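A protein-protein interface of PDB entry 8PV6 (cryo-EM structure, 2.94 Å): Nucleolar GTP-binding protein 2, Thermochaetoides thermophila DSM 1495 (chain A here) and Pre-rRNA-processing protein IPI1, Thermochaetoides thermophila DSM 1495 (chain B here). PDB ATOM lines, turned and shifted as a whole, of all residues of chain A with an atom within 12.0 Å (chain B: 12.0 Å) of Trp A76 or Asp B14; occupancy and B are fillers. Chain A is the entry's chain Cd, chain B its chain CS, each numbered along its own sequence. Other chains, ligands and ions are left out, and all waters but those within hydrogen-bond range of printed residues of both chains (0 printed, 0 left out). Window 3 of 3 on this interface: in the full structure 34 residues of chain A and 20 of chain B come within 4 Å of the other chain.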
ATOM      1  N   LYS A  67      -9.606  22.273  37.285  1.00  0.00           N
ATOM      2  CA  LYS A  67     -10.534  22.320  36.162  1.00  0.00           C
ATOM      3  C   LYS A  67     -10.177  21.202  35.192  1.00  0.00           C
ATOM      4  O   LYS A  67      -9.146  21.269  34.513  1.00  0.00           O
ATOM      5  CB  LYS A  67     -10.472  23.681  35.470  1.00  0.00           C
ATOM      6  CG  LYS A  67     -11.507  23.875  34.374  1.00  0.00           C
ATOM      7  CD  LYS A  67     -12.907  24.000  34.951  1.00  0.00           C
ATOM      8  CE  LYS A  67     -13.940  24.218  33.856  1.00  0.00           C
ATOM      9  NZ  LYS A  67     -13.754  25.526  33.170  1.00  0.00           N
ATOM     10  N   ALA A  68     -11.023  20.180  35.127  1.00  0.00           N
ATOM     11  CA  ALA A  68     -10.743  18.965  34.364  1.00  0.00           C
ATOM     12  C   ALA A  68     -11.584  18.971  33.092  1.00  0.00           C
ATOM     13  O   ALA A  68     -12.733  18.528  33.084  1.00  0.00           O
ATOM     14  CB  ALA A  68     -11.017  17.725  35.206  1.00  0.00           C
ATOM     15  N   VAL A  69     -10.998  19.477  32.010  1.00  0.00           N
ATOM     16  CA  VAL A  69     -11.607  19.436  30.688  1.00  0.00           C
ATOM     17  C   VAL A  69     -10.624  18.781  29.731  1.00  0.00           C
ATOM     18  O   VAL A  69      -9.423  18.695  30.007  1.00  0.00           O
ATOM     19  CB  VAL A  69     -12.009  20.838  30.174  1.00  0.00           C
ATOM     20  CG1 VAL A  69     -12.996  21.499  31.120  1.00  0.00           C
ATOM     21  CG2 VAL A  69     -10.778  21.710  29.989  1.00  0.00           C
ATOM     22  N   ILE A  70     -11.143  18.304  28.604  1.00  0.00           N
ATOM     23  CA  ILE A  70     -10.328  17.737  27.536  1.00  0.00           C
ATOM     24  C   ILE A  70     -10.624  18.524  26.271  1.00  0.00           C
ATOM     25  O   ILE A  70     -11.763  18.531  25.787  1.00  0.00           O
ATOM     26  CB  ILE A  70     -10.596  16.242  27.331  1.00  0.00           C
ATOM     27  CG1 ILE A  70     -10.143  15.449  28.559  1.00  0.00           C
ATOM     28  CG2 ILE A  70      -9.906  15.752  26.064  1.00  0.00           C
ATOM     29  CD1 ILE A  70     -10.062  13.963  28.334  1.00  0.00           C
ATOM     30  N   GLU A  71      -9.605  19.186  25.735  1.00  0.00           N
ATOM     31  CA  GLU A  71      -9.785  19.963  24.521  1.00  0.00           C
ATOM     32  C   GLU A  71      -9.940  19.031  23.321  1.00  0.00           C
ATOM     33  O   GLU A  71      -9.308  17.971  23.275  1.00  0.00           O
ATOM     34  CB  GLU A  71      -8.599  20.901  24.306  1.00  0.00           C
ATOM     35  CG  GLU A  71      -8.447  21.966  25.382  1.00  0.00           C
ATOM     36  CD  GLU A  71      -9.552  23.006  25.347  1.00  0.00           C
ATOM     37  OE1 GLU A  71     -10.131  23.233  24.263  1.00  0.00           O
ATOM     38  OE2 GLU A  71      -9.845  23.598  26.408  1.00  0.00           O
ATOM     39  N   PRO A  72     -10.791  19.379  22.358  1.00  0.00           N
ATOM     40  CA  PRO A  72     -10.927  18.553  21.152  1.00  0.00           C
ATOM     41  C   PRO A  72      -9.642  18.537  20.337  1.00  0.00           C
ATOM     42  O   PRO A  72      -8.935  19.542  20.237  1.00  0.00           O
ATOM     43  CB  PRO A  72     -12.072  19.226  20.387  1.00  0.00           C
ATOM     44  CG  PRO A  72     -12.183  20.595  20.966  1.00  0.00           C
ATOM     45  CD  PRO A  72     -11.775  20.473  22.393  1.00  0.00           C
ATOM     46  N   ASN A  73      -9.344  17.382  19.748  1.00  0.00           N
ATOM     47  CA  ASN A  73      -8.124  17.215  18.974  1.00  0.00           C
ATOM     48  C   ASN A  73      -8.326  16.108  17.952  1.00  0.00           C
ATOM     49  O   ASN A  73      -9.084  15.161  18.182  1.00  0.00           O
ATOM     50  CB  ASN A  73      -6.928  16.897  19.876  1.00  0.00           C
ATOM     51  CG  ASN A  73      -5.605  17.180  19.207  1.00  0.00           C
ATOM     52  OD1 ASN A  73      -4.950  16.273  18.700  1.00  0.00           O
ATOM     53  ND2 ASN A  73      -5.202  18.443  19.200  1.00  0.00           N
ATOM     54  N   ARG A  74      -7.636  16.236  16.817  1.00  0.00           N
ATOM     55  CA  ARG A  74      -7.765  15.244  15.756  1.00  0.00           C
ATOM     56  C   ARG A  74      -7.057  13.944  16.104  1.00  0.00           C
ATOM     57  O   ARG A  74      -7.453  12.877  15.623  1.00  0.00           O
ATOM     58  CB  ARG A  74      -7.211  15.800  14.446  1.00  0.00           C
ATOM     59  CG  ARG A  74      -7.989  16.971  13.887  1.00  0.00           C
ATOM     60  CD  ARG A  74      -7.271  17.586  12.702  1.00  0.00           C
ATOM     61  NE  ARG A  74      -8.097  18.570  12.015  1.00  0.00           N
ATOM     62  CZ  ARG A  74      -8.823  18.313  10.936  1.00  0.00           C
ATOM     63  NH1 ARG A  74      -8.843  17.108  10.389  1.00  0.00           N
ATOM     64  NH2 ARG A  74      -9.540  19.290  10.388  1.00  0.00           N
ATOM     65  N   LYS A  75      -6.017  14.006  16.932  1.00  0.00           N
ATOM     66  CA  LYS A  75      -5.187  12.840  17.199  1.00  0.00           C
ATOM     67  C   LYS A  75      -5.805  11.877  18.202  1.00  0.00           C
ATOM     68  O   LYS A  75      -5.238  10.804  18.429  1.00  0.00           O
ATOM     69  CB  LYS A  75      -3.806  13.282  17.684  1.00  0.00           C
ATOM     70  CG  LYS A  75      -3.148  14.309  16.779  1.00  0.00           C
ATOM     71  CD  LYS A  75      -1.659  14.426  17.045  1.00  0.00           C
ATOM     72  CE  LYS A  75      -0.947  13.106  16.802  1.00  0.00           C
ATOM     73  NZ  LYS A  75       0.505  13.197  17.112  1.00  0.00           N
ATOM     74  N   TRP A  76      -6.940  12.223  18.810  1.00  0.00           N
ATOM     75  CA  TRP A  76      -7.671  11.257  19.617  1.00  0.00           C
ATOM     76  C   TRP A  76      -8.276  10.142  18.778  1.00  0.00           C
ATOM     77  O   TRP A  76      -8.459   9.031  19.289  1.00  0.00           O
ATOM     78  CB  TRP A  76      -8.796  11.941  20.402  1.00  0.00           C
ATOM     79  CG  TRP A  76      -8.374  13.020  21.359  1.00  0.00           C
ATOM     80  CD1 TRP A  76      -8.825  14.305  21.377  1.00  0.00           C
ATOM     81  CD2 TRP A  76      -7.450  12.908  22.451  1.00  0.00           C
ATOM     82  NE1 TRP A  76      -8.233  15.004  22.397  1.00  0.00           N
ATOM     83  CE2 TRP A  76      -7.384  14.169  23.072  1.00  0.00           C
ATOM     84  CE3 TRP A  76      -6.669  11.866  22.960  1.00  0.00           C
ATOM     85  CZ2 TRP A  76      -6.570  14.417  24.171  1.00  0.00           C
ATOM     86  CZ3 TRP A  76      -5.862  12.117  24.049  1.00  0.00           C
ATOM     87  CH2 TRP A  76      -5.819  13.380  24.643  1.00  0.00           C
ATOM     88  N   PHE A  77      -8.578  10.407  17.509  1.00  0.00           N
ATOM     89  CA  PHE A  77      -9.310   9.485  16.649  1.00  0.00           C
ATOM     90  C   PHE A  77      -8.413   8.896  15.568  1.00  0.00           C
ATOM     91  O   PHE A  77      -8.866   8.633  14.453  1.00  0.00           O
ATOM     92  CB  PHE A  77     -10.516  10.180  16.019  1.00  0.00           C
ATOM     93  CG  PHE A  77     -11.373  10.923  17.003  1.00  0.00           C
ATOM     94  CD1 PHE A  77     -12.380  10.271  17.691  1.00  0.00           C
ATOM     95  CD2 PHE A  77     -11.178  12.274  17.232  1.00  0.00           C
ATOM     96  CE1 PHE A  77     -13.169  10.947  18.596  1.00  0.00           C
ATOM     97  CE2 PHE A  77     -11.963  12.954  18.137  1.00  0.00           C
ATOM     98  CZ  PHE A  77     -12.962  12.290  18.819  1.00  0.00           C
ATOM     99  N   THR A  78      -7.139   8.689  15.882  1.00  0.00           N
ATOM    100  CA  THR A  78      -6.195   8.071  14.967  1.00  0.00           C
ATOM    101  C   THR A  78      -5.570   6.851  15.627  1.00  0.00           C
ATOM    102  O   THR A  78      -5.518   6.750  16.856  1.00  0.00           O
ATOM    103  CB  THR A  78      -5.089   9.048  14.543  1.00  0.00           C
ATOM    104  OG1 THR A  78      -4.425   9.561  15.705  1.00  0.00           O
ATOM    105  CG2 THR A  78      -5.670  10.202  13.743  1.00  0.00           C
ATOM    106  N   ASN A  79      -5.113   5.917  14.798  1.00  0.00           N
ATOM    107  CA  ASN A  79      -4.387   4.763  15.305  1.00  0.00           C
ATOM    108  C   ASN A  79      -3.049   5.201  15.881  1.00  0.00           C
ATOM    109  O   ASN A  79      -2.323   5.991  15.274  1.00  0.00           O
ATOM    110  CB  ASN A  79      -4.171   3.737  14.195  1.00  0.00           C
ATOM    111  CG  ASN A  79      -5.469   3.262  13.584  1.00  0.00           C
ATOM    112  OD1 ASN A  79      -6.488   3.163  14.265  1.00  0.00           O
ATOM    113  ND2 ASN A  79      -5.438   2.958  12.293  1.00  0.00           N
ATOM    114  N   THR A  80      -2.725   4.684  17.064  1.00  0.00           N
ATOM    115  CA  THR A  80      -1.520   5.101  17.764  1.00  0.00           C
ATOM    116  C   THR A  80      -0.351   4.149  17.573  1.00  0.00           C
ATOM    117  O   THR A  80       0.797   4.572  17.722  1.00  0.00           O
ATOM    118  CB  THR A  80      -1.796   5.246  19.263  1.00  0.00           C
ATOM    119  OG1 THR A  80      -1.995   3.952  19.840  1.00  0.00           O
ATOM    120  CG2 THR A  80      -3.042   6.074  19.485  1.00  0.00           C
ATOM    121  N   ARG A  81      -0.614   2.872  17.297  1.00  0.00           N
ATOM    122  CA  ARG A  81       0.429   1.883  17.053  1.00  0.00           C
ATOM    123  C   ARG A  81      -0.041   0.965  15.935  1.00  0.00           C
ATOM    124  O   ARG A  81      -1.108   0.355  16.049  1.00  0.00           O
ATOM    125  CB  ARG A  81       0.740   1.059  18.316  1.00  0.00           C
ATOM    126  CG  ARG A  81       1.051   1.864  19.574  1.00  0.00           C
ATOM    127  CD  ARG A  81       1.522   1.006  20.724  1.00  0.00           C
ATOM    128  NE  ARG A  81       1.617   1.781  21.954  1.00  0.00           N
ATOM    129  CZ  ARG A  81       2.200   1.355  23.065  1.00  0.00           C
ATOM    130  NH1 ARG A  81       2.762   0.160  23.136  1.00  0.00           N
ATOM    131  NH2 ARG A  81       2.223   2.149  24.131  1.00  0.00           N
ATOM    132  N   LYS B   9       7.241  28.748  26.394  1.00  0.00           N
ATOM    133  CA  LYS B   9       7.850  27.429  26.273  1.00  0.00           C
ATOM    134  C   LYS B   9       7.380  26.506  27.392  1.00  0.00           C
ATOM    135  O   LYS B   9       7.653  25.305  27.376  1.00  0.00           O
ATOM    136  CB  LYS B   9       9.377  27.539  26.288  1.00  0.00           C
ATOM    137  N   GLU B  10       6.670  27.075  28.366  1.00  0.00           N
ATOM    138  CA  GLU B  10       6.166  26.306  29.497  1.00  0.00           C
ATOM    139  C   GLU B  10       4.830  25.634  29.213  1.00  0.00           C
ATOM    140  O   GLU B  10       4.338  24.898  30.077  1.00  0.00           O
ATOM    141  CB  GLU B  10       6.040  27.207  30.727  1.00  0.00           C
ATOM    142  N   LYS B  11       4.233  25.871  28.047  1.00  0.00           N
ATOM    143  CA  LYS B  11       2.962  25.244  27.715  1.00  0.00           C
ATOM    144  C   LYS B  11       3.144  23.751  27.475  1.00  0.00           C
ATOM    145  O   LYS B  11       4.138  23.313  26.888  1.00  0.00           O
ATOM    146  CB  LYS B  11       2.353  25.906  26.477  1.00  0.00           C
ATOM    147  N   GLN B  12       2.170  22.962  27.937  1.00  0.00           N
ATOM    148  CA  GLN B  12       2.197  21.507  27.813  1.00  0.00           C
ATOM    149  C   GLN B  12       0.942  21.055  27.064  1.00  0.00           C
ATOM    150  O   GLN B  12      -0.113  20.828  27.660  1.00  0.00           O
ATOM    151  CB  GLN B  12       2.305  20.838  29.183  1.00  0.00           C
ATOM    152  CG  GLN B  12       3.622  21.085  29.896  1.00  0.00           C
ATOM    153  CD  GLN B  12       3.684  20.402  31.248  1.00  0.00           C
ATOM    154  OE1 GLN B  12       2.715  19.787  31.691  1.00  0.00           O
ATOM    155  NE2 GLN B  12       4.830  20.508  31.911  1.00  0.00           N
ATOM    156  N   LYS B  13       1.062  20.930  25.745  1.00  0.00           N
ATOM    157  CA  LYS B  13      -0.042  20.430  24.943  1.00  0.00           C
ATOM    158  C   LYS B  13      -0.198  18.925  25.131  1.00  0.00           C
ATOM    159  O   LYS B  13       0.723  18.231  25.571  1.00  0.00           O
ATOM    160  CB  LYS B  13       0.181  20.752  23.465  1.00  0.00           C
ATOM    161  CG  LYS B  13       0.454  22.218  23.181  1.00  0.00           C
ATOM    162  CD  LYS B  13       0.722  22.447  21.703  1.00  0.00           C
ATOM    163  CE  LYS B  13       0.967  23.916  21.406  1.00  0.00           C
ATOM    164  NZ  LYS B  13      -0.194  24.760  21.801  1.00  0.00           N
ATOM    165  N   ASP B  14      -1.394  18.424  24.809  1.00  0.00           N
ATOM    166  CA  ASP B  14      -1.638  16.987  24.861  1.00  0.00           C
ATOM    167  C   ASP B  14      -0.804  16.240  23.830  1.00  0.00           C
ATOM    168  O   ASP B  14      -0.292  15.153  24.118  1.00  0.00           O
ATOM    169  CB  ASP B  14      -3.122  16.699  24.647  1.00  0.00           C
ATOM    170  CG  ASP B  14      -4.001  17.393  25.663  1.00  0.00           C
ATOM    171  OD1 ASP B  14      -3.526  17.634  26.791  1.00  0.00           O
ATOM    172  OD2 ASP B  14      -5.164  17.702  25.333  1.00  0.00           O
ATOM    173  N   PHE B  15      -0.659  16.802  22.633  1.00  0.00           N
ATOM    174  CA  PHE B  15       0.152  16.220  21.576  1.00  0.00           C
ATOM    175  C   PHE B  15       1.170  17.246  21.107  1.00  0.00           C
ATOM    176  O   PHE B  15       0.825  18.405  20.858  1.00  0.00           O
ATOM    177  CB  PHE B  15      -0.709  15.763  20.397  1.00  0.00           C
ATOM    178  CG  PHE B  15      -1.728  14.727  20.759  1.00  0.00           C
ATOM    179  CD1 PHE B  15      -1.409  13.382  20.717  1.00  0.00           C
ATOM    180  CD2 PHE B  15      -3.005  15.096  21.143  1.00  0.00           C
ATOM    181  CE1 PHE B  15      -2.343  12.425  21.049  1.00  0.00           C
ATOM    182  CE2 PHE B  15      -3.942  14.145  21.477  1.00  0.00           C
ATOM    183  CZ  PHE B  15      -3.610  12.808  21.429  1.00  0.00           C
ATOM    184  N   GLN B  16       2.421  16.817  20.987  1.00  0.00           N
ATOM    185  CA  GLN B  16       3.513  17.680  20.560  1.00  0.00           C
ATOM    186  C   GLN B  16       3.768  17.454  19.077  1.00  0.00           C
ATOM    187  O   GLN B  16       4.046  16.327  18.657  1.00  0.00           O
ATOM    188  CB  GLN B  16       4.779  17.409  21.372  1.00  0.00           C
ATOM    189  CG  GLN B  16       4.610  17.620  22.866  1.00  0.00           C
ATOM    190  CD  GLN B  16       5.888  17.353  23.637  1.00  0.00           C
ATOM    191  OE1 GLN B  16       6.880  16.891  23.075  1.00  0.00           O
ATOM    192  NE2 GLN B  16       5.868  17.647  24.932  1.00  0.00           N
ATOM    193  N   LYS B  17       3.669  18.522  18.294  1.00  0.00           N
ATOM    194  CA  LYS B  17       3.933  18.417  16.869  1.00  0.00           C
ATOM    195  C   LYS B  17       5.433  18.259  16.632  1.00  0.00           C
ATOM    196  O   LYS B  17       6.227  19.070  17.124  1.00  0.00           O
ATOM    197  CB  LYS B  17       3.416  19.655  16.136  1.00  0.00           C
ATOM    198  CG  LYS B  17       1.972  20.006  16.448  1.00  0.00           C
ATOM    199  CD  LYS B  17       1.485  21.152  15.579  1.00  0.00           C
ATOM    200  CE  LYS B  17      -0.015  21.356  15.724  1.00  0.00           C
ATOM    201  NZ  LYS B  17      -0.544  22.327  14.727  1.00  0.00           N
ATOM    202  N   PRO B  18       5.856  17.224  15.910  1.00  0.00           N
ATOM    203  CA  PRO B  18       7.277  17.098  15.571  1.00  0.00           C
ATOM    204  C   PRO B  18       7.717  18.198  14.619  1.00  0.00           C
ATOM    205  O   PRO B  18       6.951  18.667  13.775  1.00  0.00           O
ATOM    206  CB  PRO B  18       7.363  15.719  14.909  1.00  0.00           C
ATOM    207  CG  PRO B  18       5.992  15.479  14.372  1.00  0.00           C
ATOM    208  CD  PRO B  18       5.051  16.127  15.348  1.00  0.00           C
ATOM    209  N   SER B  30       4.650   8.477  14.160  1.00  0.00           N
ATOM    210  CA  SER B  30       4.298   8.286  15.564  1.00  0.00           C
ATOM    211  C   SER B  30       3.677   6.917  15.806  1.00  0.00           C
ATOM    212  O   SER B  30       3.778   6.369  16.909  1.00  0.00           O
ATOM    213  CB  SER B  30       3.347   9.394  16.015  1.00  0.00           C
ATOM    214  OG  SER B  30       2.301   9.577  15.077  1.00  0.00           O
ATOM    215  N   ASN B  31       3.030   6.346  14.788  1.00  0.00           N
ATOM    216  CA  ASN B  31       2.400   5.044  14.961  1.00  0.00           C
ATOM    217  C   ASN B  31       3.332   3.892  14.607  1.00  0.00           C
ATOM    218  O   ASN B  31       2.890   2.739  14.601  1.00  0.00           O
ATOM    219  CB  ASN B  31       1.112   4.964  14.138  1.00  0.00           C
ATOM    220  CG  ASN B  31       1.315   5.336  12.685  1.00  0.00           C
ATOM    221  OD1 ASN B  31       2.432   5.595  12.242  1.00  0.00           O
ATOM    222  ND2 ASN B  31       0.225   5.362  11.929  1.00  0.00           N
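The indole nitrogen of Trp A76 lies within hydrogen-bond range of the backbone carbonyl oxygen of Glu A71, 3.3 Å away. N of Lys A75 sits at hydrogen-bond distance from OD1 of Asn A73. O of Lys A75 sits at hydrogen-bond distance from OG1 of Thr A78 (3.1 Å).
Of the 15 printed residues of chain A, 6 touch a printed residue of chain B. Printed residues of chain A that touch a printed residue of chain B: Asn A73, Lys A75, Trp A76, Asn A79, Thr A80 and Arg A81. Hydrophobic or aromatic side chains of chain B that line the printed part of chain A: Phe B15.
Trp A76 touches just these residues of chain B: Asp B14 (3.8 Å) and Phe B15 (3.5 Å). Asp B14 touches just one residue of chain A: Trp A76 (3.8 Å). No residue of chain B comes within 4 Å of Ile A70. No residue of chain B comes within 4 Å of Glu A71. No residue of chain B comes within 4 Å of Phe A77. No residue of chain B comes within 4 Å of Thr A78. No residue of chain A comes within 4 Å of Lys B13. Of chain A, only Asn A73, Lys A75 and Trp A76 come within 4 Å of Phe B15. Gln B16 touches none of the printed residues of chain A. Of the printed residues of chain B, Asn A79 touches Asn B31. Printed residues of chain B within 4 Å of Arg A81: Asn B31 (3.6 Å). Printed residues of chain A within 4 Å of Ser B30: Thr A80. Glu B10 touches none of the printed residues of chain A. Gln B12 touches none of the printed residues of chain A. The nearest residue of chain A that does not touch Asp B14 is Glu A71 (4.6 Å). The nearest printed residue of chain A that does not touch Ser B30 is Lys A75 (4.5 Å).
Among the printed residues, pairs that only touch across the chains: Thr A80 with Asn B31 (3.2 Å), Asn A73 with Phe B15 (3.3 Å), Trp A76 with Phe B15 (3.5 Å), Thr A80 with Ser B30 (3.6 Å), Arg A81 with Asn B31 (3.6 Å), Lys A75 with Phe B15 (3.7 Å), Trp A76 with Asp B14 (3.8 Å) and Asn A79 with Asn B31 (3.8 Å).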
